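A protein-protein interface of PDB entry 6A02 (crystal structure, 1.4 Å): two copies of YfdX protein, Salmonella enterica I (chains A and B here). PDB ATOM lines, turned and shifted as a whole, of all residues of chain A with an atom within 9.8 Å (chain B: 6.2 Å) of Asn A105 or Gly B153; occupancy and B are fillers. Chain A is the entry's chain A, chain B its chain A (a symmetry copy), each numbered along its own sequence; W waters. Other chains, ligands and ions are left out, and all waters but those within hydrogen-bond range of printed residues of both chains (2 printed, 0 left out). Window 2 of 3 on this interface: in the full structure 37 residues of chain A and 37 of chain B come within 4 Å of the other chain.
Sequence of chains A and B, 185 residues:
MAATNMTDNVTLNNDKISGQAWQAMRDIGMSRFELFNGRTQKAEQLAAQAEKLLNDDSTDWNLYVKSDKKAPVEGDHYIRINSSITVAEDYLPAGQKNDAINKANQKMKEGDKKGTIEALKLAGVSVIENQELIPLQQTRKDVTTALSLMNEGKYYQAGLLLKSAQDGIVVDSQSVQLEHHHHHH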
ATOM      1  N   LYS A  97      -5.312  18.958  29.561  1.00  0.00           N
ATOM      2  CA  LYS A  97      -6.348  18.122  30.154  1.00  0.00           C
ATOM      3  C   LYS A  97      -7.725  18.437  29.580  1.00  0.00           C
ATOM      4  O   LYS A  97      -8.548  17.531  29.407  1.00  0.00           O
ATOM      5  CB  LYS A  97      -6.357  18.291  31.669  1.00  0.00           C
ATOM      6  CG  LYS A  97      -7.242  17.284  32.361  1.00  0.00           C
ATOM      7  CD  LYS A  97      -7.325  17.575  33.826  1.00  0.00           C
ATOM      8  CE  LYS A  97      -8.194  16.549  34.516  1.00  0.00           C
ATOM      9  NZ  LYS A  97      -8.134  16.734  35.984  1.00  0.00           N
ATOM     10  N   ASN A  98      -7.992  19.714  29.293  1.00  0.00           N
ATOM     11  CA  ASN A  98      -9.263  20.095  28.684  1.00  0.00           C
ATOM     12  C   ASN A  98      -9.475  19.364  27.366  1.00  0.00           C
ATOM     13  O   ASN A  98     -10.546  18.794  27.123  1.00  0.00           O
ATOM     14  CB  ASN A  98      -9.297  21.608  28.466  1.00  0.00           C
ATOM     15  CG  ASN A  98      -9.361  22.386  29.766  1.00  0.00           C
ATOM     16  OD1 ASN A  98      -9.610  21.828  30.824  1.00  0.00           O
ATOM     17  ND2 ASN A  98      -9.131  23.688  29.686  1.00  0.00           N
ATOM     18  N   ASP A  99      -8.462  19.370  26.499  1.00  0.00           N
ATOM     19  CA  ASP A  99      -8.597  18.705  25.209  1.00  0.00           C
ATOM     20  C   ASP A  99      -8.794  17.205  25.379  1.00  0.00           C
ATOM     21  O   ASP A  99      -9.555  16.580  24.630  1.00  0.00           O
ATOM     22  CB  ASP A  99      -7.378  19.006  24.332  1.00  0.00           C
ATOM     23  CG  ASP A  99      -7.176  20.496  24.104  1.00  0.00           C
ATOM     24  OD1 ASP A  99      -8.145  21.262  24.294  1.00  0.00           O
ATOM     25  OD2 ASP A  99      -6.052  20.903  23.736  1.00  0.00           O
ATOM     26  N   ALA A 100      -8.128  16.610  26.371  1.00  0.00           N
ATOM     27  CA  ALA A 100      -8.287  15.179  26.597  1.00  0.00           C
ATOM     28  C   ALA A 100      -9.660  14.854  27.183  1.00  0.00           C
ATOM     29  O   ALA A 100     -10.267  13.835  26.834  1.00  0.00           O
ATOM     30  CB  ALA A 100      -7.165  14.674  27.502  1.00  0.00           C
ATOM     31  N   ILE A 101     -10.162  15.710  28.075  1.00  0.00           N
ATOM     32  CA  ILE A 101     -11.493  15.492  28.637  1.00  0.00           C
ATOM     33  C   ILE A 101     -12.561  15.651  27.561  1.00  0.00           C
ATOM     34  O   ILE A 101     -13.541  14.897  27.524  1.00  0.00           O
ATOM     35  CB  ILE A 101     -11.727  16.409  29.850  1.00  0.00           C
ATOM     36  CG1 ILE A 101     -10.884  15.942  31.042  1.00  0.00           C
ATOM     37  CG2 ILE A 101     -13.197  16.422  30.228  1.00  0.00           C
ATOM     38  CD1 ILE A 101     -11.160  14.507  31.469  1.00  0.00           C
ATOM     39  N   ASN A 102     -12.375  16.614  26.655  1.00  0.00           N
ATOM     40  CA  ASN A 102     -13.336  16.800  25.574  1.00  0.00           C
ATOM     41  C   ASN A 102     -13.469  15.543  24.722  1.00  0.00           C
ATOM     42  O   ASN A 102     -14.571  15.196  24.284  1.00  0.00           O
ATOM     43  CB  ASN A 102     -12.941  17.997  24.714  1.00  0.00           C
ATOM     44  CG  ASN A 102     -13.841  18.164  23.509  1.00  0.00           C
ATOM     45  OD1 ASN A 102     -15.005  18.549  23.638  1.00  0.00           O
ATOM     46  ND2 ASN A 102     -13.310  17.860  22.328  1.00  0.00           N
ATOM     47  N   LYS A 103     -12.359  14.837  24.487  1.00  0.00           N
ATOM     48  CA  LYS A 103     -12.443  13.599  23.720  1.00  0.00           C
ATOM     49  C   LYS A 103     -13.106  12.488  24.534  1.00  0.00           C
ATOM     50  O   LYS A 103     -13.837  11.652  23.987  1.00  0.00           O
ATOM     51  CB  LYS A 103     -11.050  13.195  23.226  1.00  0.00           C
ATOM     52  CG  LYS A 103     -10.977  11.778  22.727  1.00  0.00           C
ATOM     53  CD  LYS A 103      -9.539  11.362  22.450  1.00  0.00           C
ATOM     54  CE  LYS A 103      -9.505  10.013  21.782  1.00  0.00           C
ATOM     55  NZ  LYS A 103      -8.988   9.000  22.739  1.00  0.00           N
ATOM     56  N   ALA A 104     -12.864  12.456  25.847  1.00  0.00           N
ATOM     57  CA  ALA A 104     -13.551  11.481  26.686  1.00  0.00           C
ATOM     58  C   ALA A 104     -15.060  11.685  26.634  1.00  0.00           C
ATOM     59  O   ALA A 104     -15.828  10.715  26.607  1.00  0.00           O
ATOM     60  CB  ALA A 104     -13.039  11.580  28.123  1.00  0.00           C
ATOM     61  N   ASN A 105     -15.495  12.945  26.609  1.00  0.00           N
ATOM     62  CA  ASN A 105     -16.925  13.241  26.555  1.00  0.00           C
ATOM     63  C   ASN A 105     -17.560  12.716  25.271  1.00  0.00           C
ATOM     64  O   ASN A 105     -18.706  12.250  25.282  1.00  0.00           O
ATOM     65  CB  ASN A 105     -17.144  14.743  26.718  1.00  0.00           C
ATOM     66  CG  ASN A 105     -16.986  15.191  28.157  1.00  0.00           C
ATOM     67  OD1 ASN A 105     -17.193  14.398  29.076  1.00  0.00           O
ATOM     68  ND2 ASN A 105     -16.636  16.455  28.360  1.00  0.00           N
ATOM     69  N   GLN A 106     -16.821  12.758  24.159  1.00  0.00           N
ATOM     70  CA  GLN A 106     -17.347  12.235  22.901  1.00  0.00           C
ATOM     71  C   GLN A 106     -17.584  10.731  22.974  1.00  0.00           C
ATOM     72  O   GLN A 106     -18.607  10.229  22.493  1.00  0.00           O
ATOM     73  CB  GLN A 106     -16.392  12.582  21.758  1.00  0.00           C
ATOM     74  CG  GLN A 106     -16.786  11.996  20.413  1.00  0.00           C
ATOM     75  CD  GLN A 106     -18.050  12.618  19.851  1.00  0.00           C
ATOM     76  OE1 GLN A 106     -18.369  13.776  20.139  1.00  0.00           O
ATOM     77  NE2 GLN A 106     -18.776  11.853  19.042  1.00  0.00           N
ATOM     78  N   LYS A 107     -16.654   9.991  23.584  1.00  0.00           N
ATOM     79  CA  LYS A 107     -16.822   8.547  23.700  1.00  0.00           C
ATOM     80  C   LYS A 107     -18.006   8.187  24.592  1.00  0.00           C
ATOM     81  O   LYS A 107     -18.730   7.225  24.310  1.00  0.00           O
ATOM     82  CB  LYS A 107     -15.534   7.919  24.226  1.00  0.00           C
ATOM     83  CG  LYS A 107     -14.337   8.187  23.336  1.00  0.00           C
ATOM     84  CD  LYS A 107     -14.577   7.656  21.928  1.00  0.00           C
ATOM     85  CE  LYS A 107     -13.363   7.888  21.046  1.00  0.00           C
ATOM     86  NZ  LYS A 107     -13.616   7.434  19.649  1.00  0.00           N
ATOM     87  N   MET A 108     -18.215   8.933  25.682  1.00  0.00           N
ATOM     88  CA  MET A 108     -19.397   8.679  26.505  1.00  0.00           C
ATOM     89  C   MET A 108     -20.677   8.934  25.723  1.00  0.00           C
ATOM     90  O   MET A 108     -21.614   8.128  25.773  1.00  0.00           O
ATOM     91  CB  MET A 108     -19.358   9.525  27.777  1.00  0.00           C
ATOM     92  CG  MET A 108     -18.438   8.947  28.826  1.00  0.00           C
ATOM     93  SD  MET A 108     -18.409   9.887  30.364  1.00  0.00           S
ATOM     94  CE  MET A 108     -17.252  11.169  29.910  1.00  0.00           C
ATOM     95  N   LYS A 109     -20.726  10.048  24.986  1.00  0.00           N
ATOM     96  CA  LYS A 109     -21.854  10.317  24.099  1.00  0.00           C
ATOM     97  C   LYS A 109     -22.109   9.147  23.153  1.00  0.00           C
ATOM     98  O   LYS A 109     -23.263   8.779  22.904  1.00  0.00           O
ATOM     99  CB  LYS A 109     -21.587  11.597  23.302  1.00  0.00           C
ATOM    100  CG  LYS A 109     -22.635  11.881  22.221  1.00  0.00           C
ATOM    101  CD  LYS A 109     -22.094  12.739  21.081  1.00  0.00           C
ATOM    102  CE  LYS A 109     -21.800  14.162  21.515  1.00  0.00           C
ATOM    103  NZ  LYS A 109     -21.893  15.096  20.348  1.00  0.00           N
ATOM    104  N   GLU A 110     -21.039   8.539  22.631  1.00  0.00           N
ATOM    105  CA  GLU A 110     -21.163   7.438  21.685  1.00  0.00           C
ATOM    106  C   GLU A 110     -21.477   6.102  22.345  1.00  0.00           C
ATOM    107  O   GLU A 110     -21.710   5.122  21.631  1.00  0.00           O
ATOM    108  CB  GLU A 110     -19.883   7.324  20.847  1.00  0.00           C
ATOM    109  CG  GLU A 110     -19.617   8.549  19.978  1.00  0.00           C
ATOM    110  CD  GLU A 110     -18.245   8.538  19.323  1.00  0.00           C
ATOM    111  OE1 GLU A 110     -17.471   7.579  19.537  1.00  0.00           O
ATOM    112  OE2 GLU A 110     -17.939   9.503  18.593  1.00  0.00           O
ATOM    113  N   GLY A 111     -21.496   6.026  23.674  1.00  0.00           N
ATOM    114  CA  GLY A 111     -21.741   4.745  24.309  1.00  0.00           C
ATOM    115  C   GLY A 111     -20.562   3.802  24.280  1.00  0.00           C
ATOM    116  O   GLY A 111     -20.727   2.600  24.514  1.00  0.00           O
ATOM    117  N   ASP A 112     -19.368   4.324  24.021  1.00  0.00           N
ATOM    118  CA  ASP A 112     -18.162   3.528  23.801  1.00  0.00           C
ATOM    119  C   ASP A 112     -17.412   3.452  25.126  1.00  0.00           C
ATOM    120  O   ASP A 112     -16.563   4.294  25.422  1.00  0.00           O
ATOM    121  CB  ASP A 112     -17.319   4.217  22.735  1.00  0.00           C
ATOM    122  CG  ASP A 112     -16.065   3.448  22.376  1.00  0.00           C
ATOM    123  OD1 ASP A 112     -15.795   2.383  22.971  1.00  0.00           O
ATOM    124  OD2 ASP A 112     -15.332   3.934  21.487  1.00  0.00           O
ATOM    125  N   GLY A 115     -13.579   3.051  24.696  1.00  0.00           N
ATOM    126  CA  GLY A 115     -13.024   4.312  24.246  1.00  0.00           C
ATOM    127  C   GLY A 115     -13.038   5.381  25.320  1.00  0.00           C
ATOM    128  O   GLY A 115     -12.152   6.240  25.354  1.00  0.00           O
ATOM    129  N   THR A 116     -14.043   5.348  26.204  1.00  0.00           N
ATOM    130  CA  THR A 116     -14.085   6.287  27.323  1.00  0.00           C
ATOM    131  C   THR A 116     -12.917   6.048  28.270  1.00  0.00           C
ATOM    132  O   THR A 116     -12.200   6.987  28.640  1.00  0.00           O
ATOM    133  CB  THR A 116     -15.419   6.150  28.061  1.00  0.00           C
ATOM    134  OG1 THR A 116     -16.487   6.481  27.165  1.00  0.00           O
ATOM    135  CG2 THR A 116     -15.466   7.080  29.267  1.00  0.00           C
ATOM    136  N   ILE A 117     -12.706   4.790  28.660  1.00  0.00           N
ATOM    137  CA  ILE A 117     -11.589   4.453  29.540  1.00  0.00           C
ATOM    138  C   ILE A 117     -10.269   4.877  28.915  1.00  0.00           C
ATOM    139  O   ILE A 117      -9.402   5.456  29.584  1.00  0.00           O
ATOM    140  CB  ILE A 117     -11.614   2.952  29.888  1.00  0.00           C
ATOM    141  CG1 ILE A 117     -12.948   2.580  30.541  1.00  0.00           C
ATOM    142  CG2 ILE A 117     -10.439   2.585  30.782  1.00  0.00           C
ATOM    143  CD1 ILE A 117     -13.298   3.438  31.746  1.00  0.00           C
ATOM    144  N   GLU A 118     -10.103   4.627  27.616  1.00  0.00           N
ATOM    145  CA  GLU A 118      -8.832   4.948  26.976  1.00  0.00           C
ATOM    146  C   GLU A 118      -8.635   6.456  26.847  1.00  0.00           C
ATOM    147  O   GLU A 118      -7.526   6.961  27.069  1.00  0.00           O
ATOM    148  CB  GLU A 118      -8.710   4.220  25.638  1.00  0.00           C
ATOM    149  CG  GLU A 118      -8.398   2.723  25.796  1.00  0.00           C
ATOM    150  CD  GLU A 118      -7.215   2.447  26.738  1.00  0.00           C
ATOM    151  OE1 GLU A 118      -6.154   3.098  26.588  1.00  0.00           O
ATOM    152  OE2 GLU A 118      -7.346   1.579  27.630  1.00  0.00           O
ATOM    153  N   ALA A 119      -9.696   7.198  26.515  1.00  0.00           N
ATOM    154  CA  ALA A 119      -9.577   8.653  26.453  1.00  0.00           C
ATOM    155  C   ALA A 119      -9.299   9.244  27.831  1.00  0.00           C
ATOM    156  O   ALA A 119      -8.528  10.206  27.961  1.00  0.00           O
ATOM    157  CB  ALA A 119     -10.839   9.269  25.846  1.00  0.00           C
ATOM    158  N   LEU A 120      -9.918   8.687  28.875  1.00  0.00           N
ATOM    159  CA  LEU A 120      -9.653   9.188  30.219  1.00  0.00           C
ATOM    160  C   LEU A 120      -8.205   8.950  30.627  1.00  0.00           C
ATOM    161  O   LEU A 120      -7.602   9.789  31.310  1.00  0.00           O
ATOM    162  CB  LEU A 120     -10.634   8.578  31.222  1.00  0.00           C
ATOM    163  CG  LEU A 120     -12.049   9.159  31.114  1.00  0.00           C
ATOM    164  CD1 LEU A 120     -13.008   8.407  32.022  1.00  0.00           C
ATOM    165  CD2 LEU A 120     -12.057  10.643  31.446  1.00  0.00           C
ATOM    166  N   ALA A 123      -6.192  11.631  29.528  1.00  0.00           N
ATOM    167  CA  ALA A 123      -6.413  12.782  30.391  1.00  0.00           C
ATOM    168  C   ALA A 123      -5.778  12.620  31.760  1.00  0.00           C
ATOM    169  O   ALA A 123      -5.980  13.480  32.623  1.00  0.00           O
ATOM    170  CB  ALA A 123      -7.913  13.035  30.552  1.00  0.00           C
ATOM    171  N   THR B  40     -25.410   7.972  28.579  1.00  0.00           N
ATOM    172  CA  THR B  40     -25.592   9.360  29.011  1.00  0.00           C
ATOM    173  C   THR B  40     -27.058   9.771  29.024  1.00  0.00           C
ATOM    174  O   THR B  40     -27.454  10.614  29.833  1.00  0.00           O
ATOM    175  CB  THR B  40     -24.774  10.336  28.156  1.00  0.00           C
ATOM    176  OG1 THR B  40     -25.214  10.250  26.793  1.00  0.00           O
ATOM    177  CG2 THR B  40     -23.277  10.053  28.261  1.00  0.00           C
ATOM    178  N   SER B 148     -27.481  20.734  33.039  1.00  0.00           N
ATOM    179  CA  SER B 148     -27.088  21.707  32.023  1.00  0.00           C
ATOM    180  C   SER B 148     -25.794  21.292  31.337  1.00  0.00           C
ATOM    181  O   SER B 148     -25.665  21.401  30.111  1.00  0.00           O
ATOM    182  CB  SER B 148     -26.936  23.082  32.667  1.00  0.00           C
ATOM    183  OG  SER B 148     -28.177  23.554  33.167  1.00  0.00           O
ATOM    184  N   LEU B 149     -24.816  20.819  32.111  1.00  0.00           N
ATOM    185  CA  LEU B 149     -23.575  20.337  31.517  1.00  0.00           C
ATOM    186  C   LEU B 149     -23.826  19.128  30.626  1.00  0.00           C
ATOM    187  O   LEU B 149     -23.213  19.000  29.556  1.00  0.00           O
ATOM    188  CB  LEU B 149     -22.567  19.995  32.622  1.00  0.00           C
ATOM    189  CG  LEU B 149     -22.037  21.208  33.386  1.00  0.00           C
ATOM    190  CD1 LEU B 149     -21.355  20.780  34.683  1.00  0.00           C
ATOM    191  CD2 LEU B 149     -21.067  22.011  32.520  1.00  0.00           C
ATOM    192  N   MET B 150     -24.723  18.228  31.044  1.00  0.00           N
ATOM    193  CA  MET B 150     -25.073  17.096  30.191  1.00  0.00           C
ATOM    194  C   MET B 150     -25.706  17.568  28.884  1.00  0.00           C
ATOM    195  O   MET B 150     -25.372  17.054  27.810  1.00  0.00           O
ATOM    196  CB  MET B 150     -25.995  16.129  30.933  1.00  0.00           C
ATOM    197  CG  MET B 150     -25.313  15.406  32.104  1.00  0.00           C
ATOM    198  SD  MET B 150     -26.464  14.254  32.888  1.00  0.00           S
ATOM    199  CE  MET B 150     -25.776  14.171  34.556  1.00  0.00           C
ATOM    200  N   ASN B 151     -26.594  18.562  28.953  1.00  0.00           N
ATOM    201  CA  ASN B 151     -27.178  19.111  27.726  1.00  0.00           C
ATOM    202  C   ASN B 151     -26.093  19.632  26.797  1.00  0.00           C
ATOM    203  O   ASN B 151     -26.202  19.527  25.565  1.00  0.00           O
ATOM    204  CB  ASN B 151     -28.149  20.246  28.058  1.00  0.00           C
ATOM    205  CG  ASN B 151     -29.393  19.778  28.784  1.00  0.00           C
ATOM    206  OD1 ASN B 151     -29.763  18.609  28.725  1.00  0.00           O
ATOM    207  ND2 ASN B 151     -30.045  20.700  29.477  1.00  0.00           N
ATOM    208  N   GLU B 152     -25.039  20.207  27.367  1.00  0.00           N
ATOM    209  CA  GLU B 152     -23.946  20.746  26.570  1.00  0.00           C
ATOM    210  C   GLU B 152     -22.963  19.686  26.097  1.00  0.00           C
ATOM    211  O   GLU B 152     -22.053  20.017  25.332  1.00  0.00           O
ATOM    212  CB  GLU B 152     -23.206  21.826  27.361  1.00  0.00           C
ATOM    213  CG  GLU B 152     -24.058  23.033  27.694  1.00  0.00           C
ATOM    214  CD  GLU B 152     -23.392  23.957  28.698  1.00  0.00           C
ATOM    215  OE1 GLU B 152     -22.287  23.629  29.171  1.00  0.00           O
ATOM    216  OE2 GLU B 152     -23.976  25.008  29.019  1.00  0.00           O
ATOM    217  N   GLY B 153     -23.115  18.431  26.522  1.00  0.00           N
ATOM    218  CA  GLY B 153     -22.164  17.396  26.181  1.00  0.00           C
ATOM    219  C   GLY B 153     -20.955  17.308  27.086  1.00  0.00           C
ATOM    220  O   GLY B 153     -20.021  16.565  26.765  1.00  0.00           O
ATOM    221  N   LYS B 154     -20.944  18.039  28.203  1.00  0.00           N
ATOM    222  CA  LYS B 154     -19.795  18.061  29.124  1.00  0.00           C
ATOM    223  C   LYS B 154     -20.006  17.040  30.246  1.00  0.00           C
ATOM    224  O   LYS B 154     -20.218  17.375  31.416  1.00  0.00           O
ATOM    225  CB  LYS B 154     -19.581  19.469  29.667  1.00  0.00           C
ATOM    226  CG  LYS B 154     -19.159  20.480  28.603  1.00  0.00           C
ATOM    227  CD  LYS B 154     -18.975  21.869  29.192  1.00  0.00           C
ATOM    228  CE  LYS B 154     -18.607  22.877  28.112  1.00  0.00           C
ATOM    229  NZ  LYS B 154     -19.169  24.213  28.430  1.00  0.00           N
ATOM    230  N   TYR B 155     -19.931  15.767  29.849  1.00  0.00           N
ATOM    231  CA  TYR B 155     -20.359  14.678  30.720  1.00  0.00           C
ATOM    232  C   TYR B 155     -19.413  14.483  31.896  1.00  0.00           C
ATOM    233  O   TYR B 155     -19.872  14.308  33.028  1.00  0.00           O
ATOM    234  CB  TYR B 155     -20.517  13.389  29.919  1.00  0.00           C
ATOM    235  CG  TYR B 155     -21.519  13.521  28.802  1.00  0.00           C
ATOM    236  CD1 TYR B 155     -22.863  13.727  29.073  1.00  0.00           C
ATOM    237  CD2 TYR B 155     -21.117  13.459  27.473  1.00  0.00           C
ATOM    238  CE1 TYR B 155     -23.787  13.850  28.040  1.00  0.00           C
ATOM    239  CE2 TYR B 155     -22.026  13.586  26.446  1.00  0.00           C
ATOM    240  CZ  TYR B 155     -23.355  13.784  26.739  1.00  0.00           C
ATOM    241  OH  TYR B 155     -24.282  13.911  25.721  1.00  0.00           O
ATOM    242  N   TYR B 156     -18.101  14.496  31.651  1.00  0.00           N
ATOM    243  CA  TYR B 156     -17.160  14.348  32.758  1.00  0.00           C
ATOM    244  C   TYR B 156     -17.362  15.442  33.798  1.00  0.00           C
ATOM    245  O   TYR B 156     -17.350  15.180  35.013  1.00  0.00           O
ATOM    246  CB  TYR B 156     -15.721  14.382  32.245  1.00  0.00           C
ATOM    247  CG  TYR B 156     -14.742  13.947  33.307  1.00  0.00           C
ATOM    248  CD1 TYR B 156     -14.539  12.598  33.569  1.00  0.00           C
ATOM    249  CD2 TYR B 156     -14.029  14.877  34.052  1.00  0.00           C
ATOM    250  CE1 TYR B 156     -13.652  12.181  34.554  1.00  0.00           C
ATOM    251  CE2 TYR B 156     -13.139  14.468  35.044  1.00  0.00           C
ATOM    252  CZ  TYR B 156     -12.962  13.122  35.283  1.00  0.00           C
ATOM    253  OH  TYR B 156     -12.081  12.697  36.254  1.00  0.00           O
ATOM    254  N   GLN B 157     -17.557  16.678  33.339  1.00  0.00           N
ATOM    255  CA  GLN B 157     -17.764  17.787  34.258  1.00  0.00           C
ATOM    256  C   GLN B 157     -19.065  17.622  35.034  1.00  0.00           C
ATOM    257  O   GLN B 157     -19.135  17.956  36.222  1.00  0.00           O
ATOM    258  CB  GLN B 157     -17.767  19.108  33.482  1.00  0.00           C
ATOM    259  CG  GLN B 157     -16.444  19.415  32.766  1.00  0.00           C
ATOM    260  CD  GLN B 157     -16.401  18.934  31.324  1.00  0.00           C
ATOM    261  OE1 GLN B 157     -16.861  17.844  30.992  1.00  0.00           O
ATOM    262  NE2 GLN B 157     -15.823  19.764  30.453  1.00  0.00           N
HETATM  263  O   HOH W   1     -24.211   7.573  25.854  1.00  0.00           O
HETATM  264  O   HOH W   2     -15.499  19.302  27.170  1.00  0.00           O
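No position is printed for both chains.
Of the 11 pairs that touch across the chains among the printed residues, none has its exchanged pair printed and touching as well.
OD1 of Asn A105 sits at hydrogen-bond distance from N of Tyr B155.
The side-chain amide nitrogen (ND2) of Asn A105 is in hydrogen-bond range of the side-chain amide oxygen (OE1) of Gln B157 (3.0 Å).
OD1 of Asn A105 is in hydrogen-bond range of N of Tyr B156 (2.7 Å).
OE1 of Gln B157 sits close to O of Lys B154 (3.4 Å).
OG1 of Thr A116 is in hydrogen-bond range of N of Met A108, 3.3 Å away.
The side-chain amino group of Lys B154 lies within salt-bridge range of the side-chain carboxylate of Glu B152, at 3.3 Å.
The backbone NH (N) of Lys B154 lies within hydrogen-bond range of the backbone carbonyl oxygen (O) of Leu B149, at 2.8 Å.
Among the printed residues, pairs that only touch across the chains: Asn A105 with Gly B153 (3.4 Å), Met A108 with Thr B40 (3.6 Å), Asn A105 with Lys B154 (3.6 Å), Lys A109 with Tyr B155 (3.7 Å), Leu A120 with Tyr B156 (3.8 Å), Ile A101 with Tyr B156 (3.8 Å), Met A108 with Tyr B156 (3.8 Å) and Met A108 with Tyr B155 (3.9 Å).
Water W1 lies within hydrogen-bond range of O of Met A108 (2.7 Å), N of Thr B40 (3.0 Å) and O of Lys A109 (3.3 Å).
Water W2 lies within hydrogen-bond range of the side-chain amide nitrogen (ND2) of Asn A105 (3.3 Å) and the side-chain amide nitrogen (NE2) of Gln B157 (3.3 Å).
Lys A97 touches none of the printed residues of chain B.
Of the printed residues of chain B, Ile A101 touches Tyr B156 (3.8 Å).
Of chain B, only Gly B153 (3.4 Å), Lys B154 (3.6 Å), Tyr B155 (3.2 Å), Tyr B156 (2.7 Å) and Gln B157 (3.0 Å) come within 4 Å of Asn A105.
Printed residues of chain B within 4 Å of Met A108: Thr B40 (3.6 Å), Tyr B155 (3.9 Å) and Tyr B156 (3.8 Å).
Of the printed residues of chain B, Leu A120 touches Tyr B156.
Ala A123 touches none of the printed residues of chain B.
Of the printed residues of chain A, Tyr B155 touches Asn A105, Met A108 and Lys A109.
Of the printed residues of chain A, Tyr B156 touches Ile A101, Asn A105, Met A108 and Leu A120.
The nearest residue of chain B that does not touch Asn A105 is Thr B40 (5.9 Å).
The nearest printed residue of chain A that does not touch Gln B157 is Ile A101 (4.004 Å).
Of the 23 printed residues of chain A, 5 touch a printed residue of chain B.
Hydrophobic or aromatic side chains of chain A that line the printed part of chain B: Ile A101, Met A108 and Leu A120.
Among the printed residues, no Asp or Glu carboxylate lies within 4 Å of a Lys or Arg side-chain nitrogen of the other chain.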
